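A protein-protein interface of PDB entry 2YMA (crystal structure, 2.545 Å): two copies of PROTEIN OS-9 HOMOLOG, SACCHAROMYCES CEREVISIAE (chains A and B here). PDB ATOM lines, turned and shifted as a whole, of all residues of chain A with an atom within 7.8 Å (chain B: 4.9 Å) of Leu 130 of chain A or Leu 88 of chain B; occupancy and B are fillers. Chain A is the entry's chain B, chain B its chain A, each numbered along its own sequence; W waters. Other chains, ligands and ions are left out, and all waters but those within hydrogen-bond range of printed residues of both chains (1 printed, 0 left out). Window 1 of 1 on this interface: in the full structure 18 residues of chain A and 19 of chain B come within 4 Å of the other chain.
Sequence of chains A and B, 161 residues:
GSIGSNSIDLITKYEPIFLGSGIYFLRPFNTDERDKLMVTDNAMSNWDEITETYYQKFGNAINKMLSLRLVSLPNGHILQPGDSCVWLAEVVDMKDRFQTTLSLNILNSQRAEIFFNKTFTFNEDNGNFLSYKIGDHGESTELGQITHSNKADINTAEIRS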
ATOM      1  N   CYS A  85     -17.923  -4.804   2.921  1.00  0.00           N
ATOM      2  CA  CYS A  85     -17.947  -4.237   4.266  1.00  0.00           C
ATOM      3  C   CYS A  85     -16.610  -3.663   4.705  1.00  0.00           C
ATOM      4  O   CYS A  85     -15.593  -3.817   4.025  1.00  0.00           O
ATOM      5  CB  CYS A  85     -18.358  -5.318   5.260  1.00  0.00           C
ATOM      6  SG  CYS A  85     -17.078  -6.601   5.486  1.00  0.00           S
ATOM      7  N   VAL A  86     -16.637  -2.985   5.847  1.00  0.00           N
ATOM      8  CA  VAL A  86     -15.432  -2.614   6.575  1.00  0.00           C
ATOM      9  C   VAL A  86     -15.566  -3.165   7.981  1.00  0.00           C
ATOM     10  O   VAL A  86     -16.404  -2.688   8.757  1.00  0.00           O
ATOM     11  CB  VAL A  86     -15.205  -1.075   6.625  1.00  0.00           C
ATOM     12  CG1 VAL A  86     -14.016  -0.722   7.532  1.00  0.00           C
ATOM     13  CG2 VAL A  86     -14.964  -0.532   5.225  1.00  0.00           C
ATOM     14  N   TRP A  87     -14.737  -4.167   8.288  1.00  0.00           N
ATOM     15  CA  TRP A  87     -14.788  -4.905   9.550  1.00  0.00           C
ATOM     16  C   TRP A  87     -13.461  -4.691  10.261  1.00  0.00           C
ATOM     17  O   TRP A  87     -12.408  -4.763   9.634  1.00  0.00           O
ATOM     18  CB  TRP A  87     -15.033  -6.401   9.257  1.00  0.00           C
ATOM     19  CG  TRP A  87     -15.162  -7.334  10.455  1.00  0.00           C
ATOM     20  CD1 TRP A  87     -16.302  -7.618  11.162  1.00  0.00           C
ATOM     21  CD2 TRP A  87     -14.122  -8.143  11.035  1.00  0.00           C
ATOM     22  NE1 TRP A  87     -16.029  -8.537  12.160  1.00  0.00           N
ATOM     23  CE2 TRP A  87     -14.701  -8.872  12.102  1.00  0.00           C
ATOM     24  CE3 TRP A  87     -12.760  -8.319  10.760  1.00  0.00           C
ATOM     25  CZ2 TRP A  87     -13.959  -9.754  12.895  1.00  0.00           C
ATOM     26  CZ3 TRP A  87     -12.029  -9.193  11.553  1.00  0.00           C
ATOM     27  CH2 TRP A  87     -12.630  -9.901  12.604  1.00  0.00           C
ATOM     28  N   LEU A  88     -13.519  -4.416  11.562  1.00  0.00           N
ATOM     29  CA  LEU A  88     -12.337  -4.135  12.383  1.00  0.00           C
ATOM     30  C   LEU A  88     -12.287  -5.019  13.602  1.00  0.00           C
ATOM     31  O   LEU A  88     -13.345  -5.382  14.154  1.00  0.00           O
ATOM     32  CB  LEU A  88     -12.406  -2.741  12.976  1.00  0.00           C
ATOM     33  CG  LEU A  88     -12.618  -1.438  12.262  1.00  0.00           C
ATOM     34  CD1 LEU A  88     -13.965  -1.403  11.590  1.00  0.00           C
ATOM     35  CD2 LEU A  88     -12.532  -0.441  13.386  1.00  0.00           C
ATOM     36  N   SER A 103      -7.898  -3.844  10.040  1.00  0.00           N
ATOM     37  CA  SER A 103      -9.003  -3.349   9.211  1.00  0.00           C
ATOM     38  C   SER A 103      -9.156  -4.305   8.036  1.00  0.00           C
ATOM     39  O   SER A 103      -8.177  -4.626   7.357  1.00  0.00           O
ATOM     40  CB  SER A 103      -8.738  -1.909   8.738  1.00  0.00           C
ATOM     41  OG  SER A 103      -9.442  -1.593   7.546  1.00  0.00           O
ATOM     42  N   LEU A 104     -10.376  -4.780   7.818  1.00  0.00           N
ATOM     43  CA  LEU A 104     -10.669  -5.701   6.728  1.00  0.00           C
ATOM     44  C   LEU A 104     -11.705  -5.071   5.818  1.00  0.00           C
ATOM     45  O   LEU A 104     -12.849  -4.855   6.222  1.00  0.00           O
ATOM     46  CB  LEU A 104     -11.195  -7.049   7.249  1.00  0.00           C
ATOM     47  CG  LEU A 104     -11.935  -7.914   6.207  1.00  0.00           C
ATOM     48  CD1 LEU A 104     -11.063  -8.269   5.015  1.00  0.00           C
ATOM     49  CD2 LEU A 104     -12.505  -9.177   6.820  1.00  0.00           C
ATOM     50  N   PHE A 120      -4.745   2.890  15.729  1.00  0.00           N
ATOM     51  CA  PHE A 120      -6.181   3.028  15.842  1.00  0.00           C
ATOM     52  C   PHE A 120      -6.687   2.265  17.065  1.00  0.00           C
ATOM     53  O   PHE A 120      -6.688   1.036  17.092  1.00  0.00           O
ATOM     54  CB  PHE A 120      -6.898   2.573  14.574  1.00  0.00           C
ATOM     55  CG  PHE A 120      -8.327   2.999  14.531  1.00  0.00           C
ATOM     56  CD1 PHE A 120      -9.296   2.274  15.204  1.00  0.00           C
ATOM     57  CD2 PHE A 120      -8.697   4.152  13.860  1.00  0.00           C
ATOM     58  CE1 PHE A 120     -10.609   2.676  15.191  1.00  0.00           C
ATOM     59  CE2 PHE A 120     -10.008   4.556  13.837  1.00  0.00           C
ATOM     60  CZ  PHE A 120     -10.967   3.816  14.507  1.00  0.00           C
ATOM     61  N   PHE A 122      -9.825   1.284  19.592  1.00  0.00           N
ATOM     62  CA  PHE A 122     -11.273   1.099  19.678  1.00  0.00           C
ATOM     63  C   PHE A 122     -11.889   1.736  20.913  1.00  0.00           C
ATOM     64  O   PHE A 122     -11.364   1.624  22.020  1.00  0.00           O
ATOM     65  CB  PHE A 122     -11.570  -0.375  19.792  1.00  0.00           C
ATOM     66  CG  PHE A 122     -11.952  -1.035  18.508  1.00  0.00           C
ATOM     67  CD1 PHE A 122     -13.222  -0.864  17.972  1.00  0.00           C
ATOM     68  CD2 PHE A 122     -11.062  -1.886  17.872  1.00  0.00           C
ATOM     69  CE1 PHE A 122     -13.593  -1.513  16.814  1.00  0.00           C
ATOM     70  CE2 PHE A 122     -11.417  -2.540  16.716  1.00  0.00           C
ATOM     71  CZ  PHE A 122     -12.689  -2.354  16.184  1.00  0.00           C
ATOM     72  N   ASN A 126     -17.860   0.189  20.669  1.00  0.00           N
ATOM     73  CA  ASN A 126     -17.901  -0.165  19.258  1.00  0.00           C
ATOM     74  C   ASN A 126     -18.100  -1.658  19.017  1.00  0.00           C
ATOM     75  O   ASN A 126     -17.554  -2.492  19.736  1.00  0.00           O
ATOM     76  CB  ASN A 126     -16.640   0.315  18.531  1.00  0.00           C
ATOM     77  CG  ASN A 126     -16.482   1.822  18.576  1.00  0.00           C
ATOM     78  OD1 ASN A 126     -17.459   2.564  18.481  1.00  0.00           O
ATOM     79  ND2 ASN A 126     -15.250   2.282  18.730  1.00  0.00           N
ATOM     80  N   GLY A 127     -18.887  -1.981  17.994  1.00  0.00           N
ATOM     81  CA  GLY A 127     -18.876  -3.301  17.396  1.00  0.00           C
ATOM     82  C   GLY A 127     -17.750  -3.421  16.380  1.00  0.00           C
ATOM     83  O   GLY A 127     -16.919  -2.517  16.268  1.00  0.00           O
ATOM     84  N   ASN A 128     -17.726  -4.534  15.645  1.00  0.00           N
ATOM     85  CA  ASN A 128     -16.674  -4.804  14.657  1.00  0.00           C
ATOM     86  C   ASN A 128     -16.894  -4.108  13.314  1.00  0.00           C
ATOM     87  O   ASN A 128     -15.941  -3.813  12.600  1.00  0.00           O
ATOM     88  CB  ASN A 128     -16.484  -6.320  14.438  1.00  0.00           C
ATOM     89  CG  ASN A 128     -16.067  -7.043  15.709  1.00  0.00           C
ATOM     90  OD1 ASN A 128     -16.887  -7.686  16.368  1.00  0.00           O
ATOM     91  ND2 ASN A 128     -14.795  -6.914  16.074  1.00  0.00           N
ATOM     92  N   PHE A 129     -18.150  -3.858  12.961  1.00  0.00           N
ATOM     93  CA  PHE A 129     -18.453  -3.246  11.668  1.00  0.00           C
ATOM     94  C   PHE A 129     -18.506  -1.728  11.713  1.00  0.00           C
ATOM     95  O   PHE A 129     -19.287  -1.135  12.471  1.00  0.00           O
ATOM     96  CB  PHE A 129     -19.779  -3.744  11.121  1.00  0.00           C
ATOM     97  CG  PHE A 129     -19.752  -5.162  10.661  1.00  0.00           C
ATOM     98  CD1 PHE A 129     -19.412  -5.468   9.346  1.00  0.00           C
ATOM     99  CD2 PHE A 129     -20.082  -6.197  11.533  1.00  0.00           C
ATOM    100  CE1 PHE A 129     -19.399  -6.786   8.904  1.00  0.00           C
ATOM    101  CE2 PHE A 129     -20.069  -7.531  11.099  1.00  0.00           C
ATOM    102  CZ  PHE A 129     -19.729  -7.826   9.784  1.00  0.00           C
ATOM    103  N   LEU A 130     -17.667  -1.113  10.885  1.00  0.00           N
ATOM    104  CA  LEU A 130     -17.748   0.309  10.647  1.00  0.00           C
ATOM    105  C   LEU A 130     -18.815   0.550   9.577  1.00  0.00           C
ATOM    106  O   LEU A 130     -19.657   1.437   9.715  1.00  0.00           O
ATOM    107  CB  LEU A 130     -16.395   0.838  10.200  1.00  0.00           C
ATOM    108  CG  LEU A 130     -16.429   2.290   9.742  1.00  0.00           C
ATOM    109  CD1 LEU A 130     -16.964   3.190  10.872  1.00  0.00           C
ATOM    110  CD2 LEU A 130     -15.028   2.698   9.302  1.00  0.00           C
ATOM    111  N   SER A 131     -18.792  -0.264   8.525  1.00  0.00           N
ATOM    112  CA  SER A 131     -19.818  -0.192   7.495  1.00  0.00           C
ATOM    113  C   SER A 131     -20.050  -1.546   6.805  1.00  0.00           C
ATOM    114  O   SER A 131     -19.237  -2.459   6.918  1.00  0.00           O
ATOM    115  CB  SER A 131     -19.466   0.900   6.475  1.00  0.00           C
ATOM    116  OG  SER A 131     -18.785   0.387   5.344  1.00  0.00           O
ATOM    117  N   TYR A 132     -21.164  -1.676   6.091  1.00  0.00           N
ATOM    118  CA  TYR A 132     -21.401  -2.879   5.305  1.00  0.00           C
ATOM    119  C   TYR A 132     -22.401  -2.600   4.192  1.00  0.00           C
ATOM    120  O   TYR A 132     -23.076  -1.563   4.185  1.00  0.00           O
ATOM    121  CB  TYR A 132     -21.902  -4.021   6.203  1.00  0.00           C
ATOM    122  CG  TYR A 132     -23.189  -3.664   6.898  1.00  0.00           C
ATOM    123  CD1 TYR A 132     -24.415  -3.806   6.245  1.00  0.00           C
ATOM    124  CD2 TYR A 132     -23.178  -3.130   8.190  1.00  0.00           C
ATOM    125  CE1 TYR A 132     -25.606  -3.446   6.869  1.00  0.00           C
ATOM    126  CE2 TYR A 132     -24.362  -2.762   8.822  1.00  0.00           C
ATOM    127  CZ  TYR A 132     -25.571  -2.926   8.158  1.00  0.00           C
ATOM    128  OH  TYR A 132     -26.745  -2.568   8.786  1.00  0.00           O
ATOM    129  N   VAL B  86     -10.211   4.176   3.908  1.00  0.00           N
ATOM    130  CA  VAL B  86     -11.378   4.275   4.754  1.00  0.00           C
ATOM    131  C   VAL B  86     -11.181   5.485   5.660  1.00  0.00           C
ATOM    132  O   VAL B  86     -10.266   5.517   6.499  1.00  0.00           O
ATOM    133  CB  VAL B  86     -11.615   3.010   5.612  1.00  0.00           C
ATOM    134  CG1 VAL B  86     -12.732   3.268   6.615  1.00  0.00           C
ATOM    135  CG2 VAL B  86     -11.977   1.859   4.728  1.00  0.00           C
ATOM    136  N   TRP B  87     -12.039   6.481   5.464  1.00  0.00           N
ATOM    137  CA  TRP B  87     -11.913   7.775   6.122  1.00  0.00           C
ATOM    138  C   TRP B  87     -13.176   8.004   6.947  1.00  0.00           C
ATOM    139  O   TRP B  87     -14.287   7.765   6.463  1.00  0.00           O
ATOM    140  CB  TRP B  87     -11.729   8.869   5.053  1.00  0.00           C
ATOM    141  CG  TRP B  87     -11.568  10.295   5.572  1.00  0.00           C
ATOM    142  CD1 TRP B  87     -10.398  10.914   5.955  1.00  0.00           C
ATOM    143  CD2 TRP B  87     -12.604  11.275   5.735  1.00  0.00           C
ATOM    144  NE1 TRP B  87     -10.652  12.210   6.346  1.00  0.00           N
ATOM    145  CE2 TRP B  87     -11.992  12.457   6.222  1.00  0.00           C
ATOM    146  CE3 TRP B  87     -13.991  11.271   5.515  1.00  0.00           C
ATOM    147  CZ2 TRP B  87     -12.722  13.620   6.498  1.00  0.00           C
ATOM    148  CZ3 TRP B  87     -14.715  12.433   5.785  1.00  0.00           C
ATOM    149  CH2 TRP B  87     -14.078  13.588   6.276  1.00  0.00           C
ATOM    150  N   LEU B  88     -13.015   8.444   8.192  1.00  0.00           N
ATOM    151  CA  LEU B  88     -14.151   8.594   9.110  1.00  0.00           C
ATOM    152  C   LEU B  88     -14.180   9.984   9.691  1.00  0.00           C
ATOM    153  O   LEU B  88     -13.135  10.571   9.956  1.00  0.00           O
ATOM    154  CB  LEU B  88     -14.030   7.664  10.326  1.00  0.00           C
ATOM    155  CG  LEU B  88     -13.741   6.177  10.330  1.00  0.00           C
ATOM    156  CD1 LEU B  88     -12.374   5.892   9.728  1.00  0.00           C
ATOM    157  CD2 LEU B  88     -13.792   5.737  11.784  1.00  0.00           C
ATOM    158  N   ALA B  89     -15.380  10.475   9.966  1.00  0.00           N
ATOM    159  CA  ALA B  89     -15.541  11.775  10.599  1.00  0.00           C
ATOM    160  C   ALA B  89     -16.865  11.851  11.342  1.00  0.00           C
ATOM    161  O   ALA B  89     -17.885  11.301  10.886  1.00  0.00           O
ATOM    162  CB  ALA B  89     -15.446  12.891   9.551  1.00  0.00           C
ATOM    163  N   GLU B  90     -16.844  12.514  12.497  1.00  0.00           N
ATOM    164  CA  GLU B  90     -18.076  12.831  13.204  1.00  0.00           C
ATOM    165  C   GLU B  90     -18.871  13.828  12.377  1.00  0.00           C
ATOM    166  O   GLU B  90     -18.313  14.765  11.784  1.00  0.00           O
ATOM    167  CB  GLU B  90     -17.797  13.452  14.576  1.00  0.00           C
ATOM    168  CG  GLU B  90     -17.037  12.571  15.548  1.00  0.00           C
ATOM    169  CD  GLU B  90     -16.931  13.202  16.930  1.00  0.00           C
ATOM    170  OE1 GLU B  90     -17.666  14.178  17.202  1.00  0.00           O
ATOM    171  OE2 GLU B  90     -16.117  12.720  17.746  1.00  0.00           O
ATOM    172  N   THR B 101     -21.664   9.047  12.606  1.00  0.00           N
ATOM    173  CA  THR B 101     -20.316   8.965  12.081  1.00  0.00           C
ATOM    174  C   THR B 101     -20.425   8.667  10.586  1.00  0.00           C
ATOM    175  O   THR B 101     -21.199   7.799  10.164  1.00  0.00           O
ATOM    176  CB  THR B 101     -19.457   7.913  12.848  1.00  0.00           C
ATOM    177  OG1 THR B 101     -19.132   8.420  14.154  1.00  0.00           O
ATOM    178  CG2 THR B 101     -18.171   7.623  12.116  1.00  0.00           C
ATOM    179  N   LEU B 102     -19.683   9.429   9.788  1.00  0.00           N
ATOM    180  CA  LEU B 102     -19.639   9.199   8.353  1.00  0.00           C
ATOM    181  C   LEU B 102     -18.460   8.289   8.043  1.00  0.00           C
ATOM    182  O   LEU B 102     -17.329   8.546   8.454  1.00  0.00           O
ATOM    183  CB  LEU B 102     -19.509  10.530   7.602  1.00  0.00           C
ATOM    184  CG  LEU B 102     -19.740  10.643   6.086  1.00  0.00           C
ATOM    185  CD1 LEU B 102     -18.449  10.733   5.366  1.00  0.00           C
ATOM    186  CD2 LEU B 102     -20.573   9.515   5.510  1.00  0.00           C
ATOM    187  N   SER B 103     -18.745   7.203   7.344  1.00  0.00           N
ATOM    188  CA  SER B 103     -17.705   6.327   6.842  1.00  0.00           C
ATOM    189  C   SER B 103     -17.602   6.515   5.336  1.00  0.00           C
ATOM    190  O   SER B 103     -18.585   6.331   4.614  1.00  0.00           O
ATOM    191  CB  SER B 103     -18.044   4.867   7.170  1.00  0.00           C
ATOM    192  OG  SER B 103     -17.135   3.971   6.551  1.00  0.00           O
ATOM    193  N   PHE B 115     -21.392   5.491   4.376  1.00  0.00           N
ATOM    194  CA  PHE B 115     -22.225   4.781   5.323  1.00  0.00           C
ATOM    195  C   PHE B 115     -22.352   5.682   6.532  1.00  0.00           C
ATOM    196  O   PHE B 115     -21.373   6.292   6.967  1.00  0.00           O
ATOM    197  CB  PHE B 115     -21.567   3.448   5.705  1.00  0.00           C
ATOM    198  CG  PHE B 115     -22.372   2.597   6.686  1.00  0.00           C
ATOM    199  CD1 PHE B 115     -22.199   2.739   8.062  1.00  0.00           C
ATOM    200  CD2 PHE B 115     -23.261   1.627   6.228  1.00  0.00           C
ATOM    201  CE1 PHE B 115     -22.921   1.951   8.967  1.00  0.00           C
ATOM    202  CE2 PHE B 115     -23.986   0.826   7.126  1.00  0.00           C
ATOM    203  CZ  PHE B 115     -23.821   0.994   8.497  1.00  0.00           C
ATOM    204  N   ASN B 117     -23.081   5.745  10.435  1.00  0.00           N
ATOM    205  CA  ASN B 117     -23.048   4.836  11.565  1.00  0.00           C
ATOM    206  C   ASN B 117     -23.316   5.603  12.859  1.00  0.00           C
ATOM    207  O   ASN B 117     -22.407   6.231  13.427  1.00  0.00           O
ATOM    208  CB  ASN B 117     -21.700   4.103  11.622  1.00  0.00           C
ATOM    209  CG  ASN B 117     -21.713   2.923  12.591  1.00  0.00           C
ATOM    210  OD1 ASN B 117     -22.400   2.944  13.622  1.00  0.00           O
ATOM    211  ND2 ASN B 117     -20.951   1.888  12.261  1.00  0.00           N
ATOM    212  N   PHE B 120     -21.249   4.310  16.101  1.00  0.00           N
ATOM    213  CA  PHE B 120     -19.799   4.293  16.157  1.00  0.00           C
ATOM    214  C   PHE B 120     -19.215   5.562  16.780  1.00  0.00           C
ATOM    215  O   PHE B 120     -19.281   6.644  16.205  1.00  0.00           O
ATOM    216  CB  PHE B 120     -19.182   4.048  14.785  1.00  0.00           C
ATOM    217  CG  PHE B 120     -17.742   3.657  14.858  1.00  0.00           C
ATOM    218  CD1 PHE B 120     -16.758   4.623  14.980  1.00  0.00           C
ATOM    219  CD2 PHE B 120     -17.377   2.320  14.866  1.00  0.00           C
ATOM    220  CE1 PHE B 120     -15.434   4.263  15.074  1.00  0.00           C
ATOM    221  CE2 PHE B 120     -16.055   1.951  14.954  1.00  0.00           C
ATOM    222  CZ  PHE B 120     -15.078   2.924  15.057  1.00  0.00           C
ATOM    223  N   PHE B 122     -15.992   7.731  18.302  1.00  0.00           N
ATOM    224  CA  PHE B 122     -14.557   7.927  18.190  1.00  0.00           C
ATOM    225  C   PHE B 122     -13.864   7.951  19.542  1.00  0.00           C
ATOM    226  O   PHE B 122     -14.388   8.490  20.519  1.00  0.00           O
ATOM    227  CB  PHE B 122     -14.272   9.261  17.508  1.00  0.00           C
ATOM    228  CG  PHE B 122     -14.054   9.163  16.031  1.00  0.00           C
ATOM    229  CD1 PHE B 122     -12.840   8.728  15.535  1.00  0.00           C
ATOM    230  CD2 PHE B 122     -15.050   9.527  15.139  1.00  0.00           C
ATOM    231  CE1 PHE B 122     -12.619   8.649  14.177  1.00  0.00           C
ATOM    232  CE2 PHE B 122     -14.832   9.453  13.774  1.00  0.00           C
ATOM    233  CZ  PHE B 122     -13.612   9.015  13.297  1.00  0.00           C
ATOM    234  N   ASN B 128      -8.617  10.562  11.382  1.00  0.00           N
ATOM    235  CA  ASN B 128      -9.711  10.340  10.450  1.00  0.00           C
ATOM    236  C   ASN B 128      -9.548   9.064   9.632  1.00  0.00           C
ATOM    237  O   ASN B 128     -10.530   8.531   9.115  1.00  0.00           O
ATOM    238  CB  ASN B 128      -9.844  11.543   9.486  1.00  0.00           C
ATOM    239  CG  ASN B 128     -10.331  12.813  10.182  1.00  0.00           C
ATOM    240  OD1 ASN B 128      -9.553  13.743  10.422  1.00  0.00           O
ATOM    241  ND2 ASN B 128     -11.628  12.856  10.511  1.00  0.00           N
ATOM    242  N   PHE B 129      -8.316   8.592   9.473  1.00  0.00           N
ATOM    243  CA  PHE B 129      -8.083   7.388   8.674  1.00  0.00           C
ATOM    244  C   PHE B 129      -8.015   6.125   9.499  1.00  0.00           C
ATOM    245  O   PHE B 129      -7.285   6.042  10.480  1.00  0.00           O
ATOM    246  CB  PHE B 129      -6.817   7.494   7.845  1.00  0.00           C
ATOM    247  CG  PHE B 129      -6.928   8.433   6.700  1.00  0.00           C
ATOM    248  CD1 PHE B 129      -7.398   7.997   5.477  1.00  0.00           C
ATOM    249  CD2 PHE B 129      -6.552   9.760   6.841  1.00  0.00           C
ATOM    250  CE1 PHE B 129      -7.490   8.880   4.406  1.00  0.00           C
ATOM    251  CE2 PHE B 129      -6.625  10.631   5.776  1.00  0.00           C
ATOM    252  CZ  PHE B 129      -7.101  10.195   4.562  1.00  0.00           C
ATOM    253  N   LEU B 130      -8.804   5.142   9.092  1.00  0.00           N
ATOM    254  CA  LEU B 130      -8.690   3.801   9.632  1.00  0.00           C
ATOM    255  C   LEU B 130      -7.636   3.058   8.803  1.00  0.00           C
ATOM    256  O   LEU B 130      -6.792   2.338   9.345  1.00  0.00           O
ATOM    257  CB  LEU B 130     -10.040   3.085   9.566  1.00  0.00           C
ATOM    258  CG  LEU B 130     -10.012   1.602   9.923  1.00  0.00           C
ATOM    259  CD1 LEU B 130      -9.454   1.411  11.326  1.00  0.00           C
ATOM    260  CD2 LEU B 130     -11.391   1.004   9.787  1.00  0.00           C
HETATM  261  O   HOH W   1     -18.158   3.109   4.095  1.00  0.00           O
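The side-chain amide nitrogen (ND2) of Asn 117 of chain B sits at hydrogen-bond distance from the backbone carbonyl oxygen (O) of Phe 129 of chain A (3.5 Å).
The side-chain amide nitrogen (ND2) of Asn 117 of chain B is in hydrogen-bond range of the backbone carbonyl oxygen (O) of Leu 130 of chain A (2.9 Å).
Of the printed residues of chain B, Val 86 of chain A touches Val 86 and Leu 130.
Printed residues of chain B within 4 Å of Leu 88 of chain A: Leu 130.
Leu 130 of chain A touches just these residues of chain B: Val 86 (3.6 Å), Leu 88 (3.8 Å), Ser 103 (3.7 Å), Phe 115 (3.3 Å) and Asn 117 (2.9 Å).
Leu 88 of chain B touches just one residue of chain A: Leu 130 (3.8 Å).
Printed residues of chain A within 4 Å of Phe 115 of chain B: Leu 130 (3.3 Å), Ser 131 (3.4 Å) and Tyr 132 (3.8 Å).
Of the printed residues of chain A, Asn 117 of chain B touches Phe 129 (3.5 Å) and Leu 130 (2.9 Å).
The nearest residue of chain B that does not touch Leu 130 of chain A is Leu 130 of chain B (4.04 Å).
Val 86 of chain B touches its own counterpart, Val 86 of chain A.
Leu 88 of chain A touches Leu 130 of chain B, and with the chains exchanged Leu 130 of chain A touches Leu 88 of chain B.
Ser 103 of chain A touches Leu 130 of chain B, and with the chains exchanged Leu 130 of chain A touches Ser 103 of chain B.
Phe 120 of chain A touches Leu 130 of chain B, but with the chains exchanged Leu 130 of chain A does not touch Phe 120 of chain B (4.1 Å).
9 positions are printed for both chains.
Of the 15 pairs that touch across the chains among the printed residues, 7 have their exchanged pair printed and touching as well.
Water W1 lies within hydrogen-bond range of OG of Ser 103 of chain B (2.8 Å) and OG of Ser 131 of chain A (3.1 Å).
O of Phe 120 of chain B sits at hydrogen-bond distance from OG1 of Thr 101 of chain B.
The backbone carbonyl oxygen (O) of Phe 115 of chain B sits at hydrogen-bond distance from the backbone NH (N) of Ser 103 of chain B (2.8 Å).
OD1 of Asn 117 of chain B lies within hydrogen-bond range of N of Phe 120 of chain B.
The backbone carbonyl oxygen of Val 86 of chain A sits at hydrogen-bond distance from the backbone NH of Leu 130 of chain A (2.9 Å).
N of Val 86 of chain A lies within hydrogen-bond range of O of Ser 131 of chain A (2.9 Å).
The backbone NH (N) of Leu 88 of chain A sits at hydrogen-bond distance from the backbone carbonyl oxygen (O) of Asn 128 of chain A (2.7 Å).
Hydrophobic or aromatic side chains of chain A within 4 Å of the printed part of chain B: Val 86, Leu 88, Phe 120, Leu 130 and Tyr 132.
Printed residues of chain B that touch a printed residue of chain A: Val 86, Leu 88, Ser 103, Phe 115, Asn 117, Phe 120 and Leu 130.
Among the printed residues, 15 pairs touch across the chains.
Among the printed residues, no Asp or Glu carboxylate lies within 4 Å of a Lys or Arg side-chain nitrogen of the other chain.
Val 86 of chain B touches Val 86 of chain A.
Val 86 of chain A touches Leu 130 of chain B (CG1 to CD2, 3.9 Å).
Leu 88 of chain A touches Leu 130 of chain B (CG to CD2, 3.7 Å).
CG of Leu 130 of chain B touches CB of Ser 103 of chain A, 3.9 Å away.
CG of Phe 120 of chain A touches CD1 of Leu 130 of chain B, at 3.8 Å.
CD2 of Leu 130 of chain A touches CG1 of Val 86 of chain B, 3.6 Å away.
Leu 130 of chain A touches Leu 88 of chain B.
Leu 130 of chain A touches Ser 103 of chain B.
CD1 of Phe 115 of chain B touches O of Leu 130 of chain A (3.3 Å).
Ser 103 of chain B touches Ser 131 of chain A.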
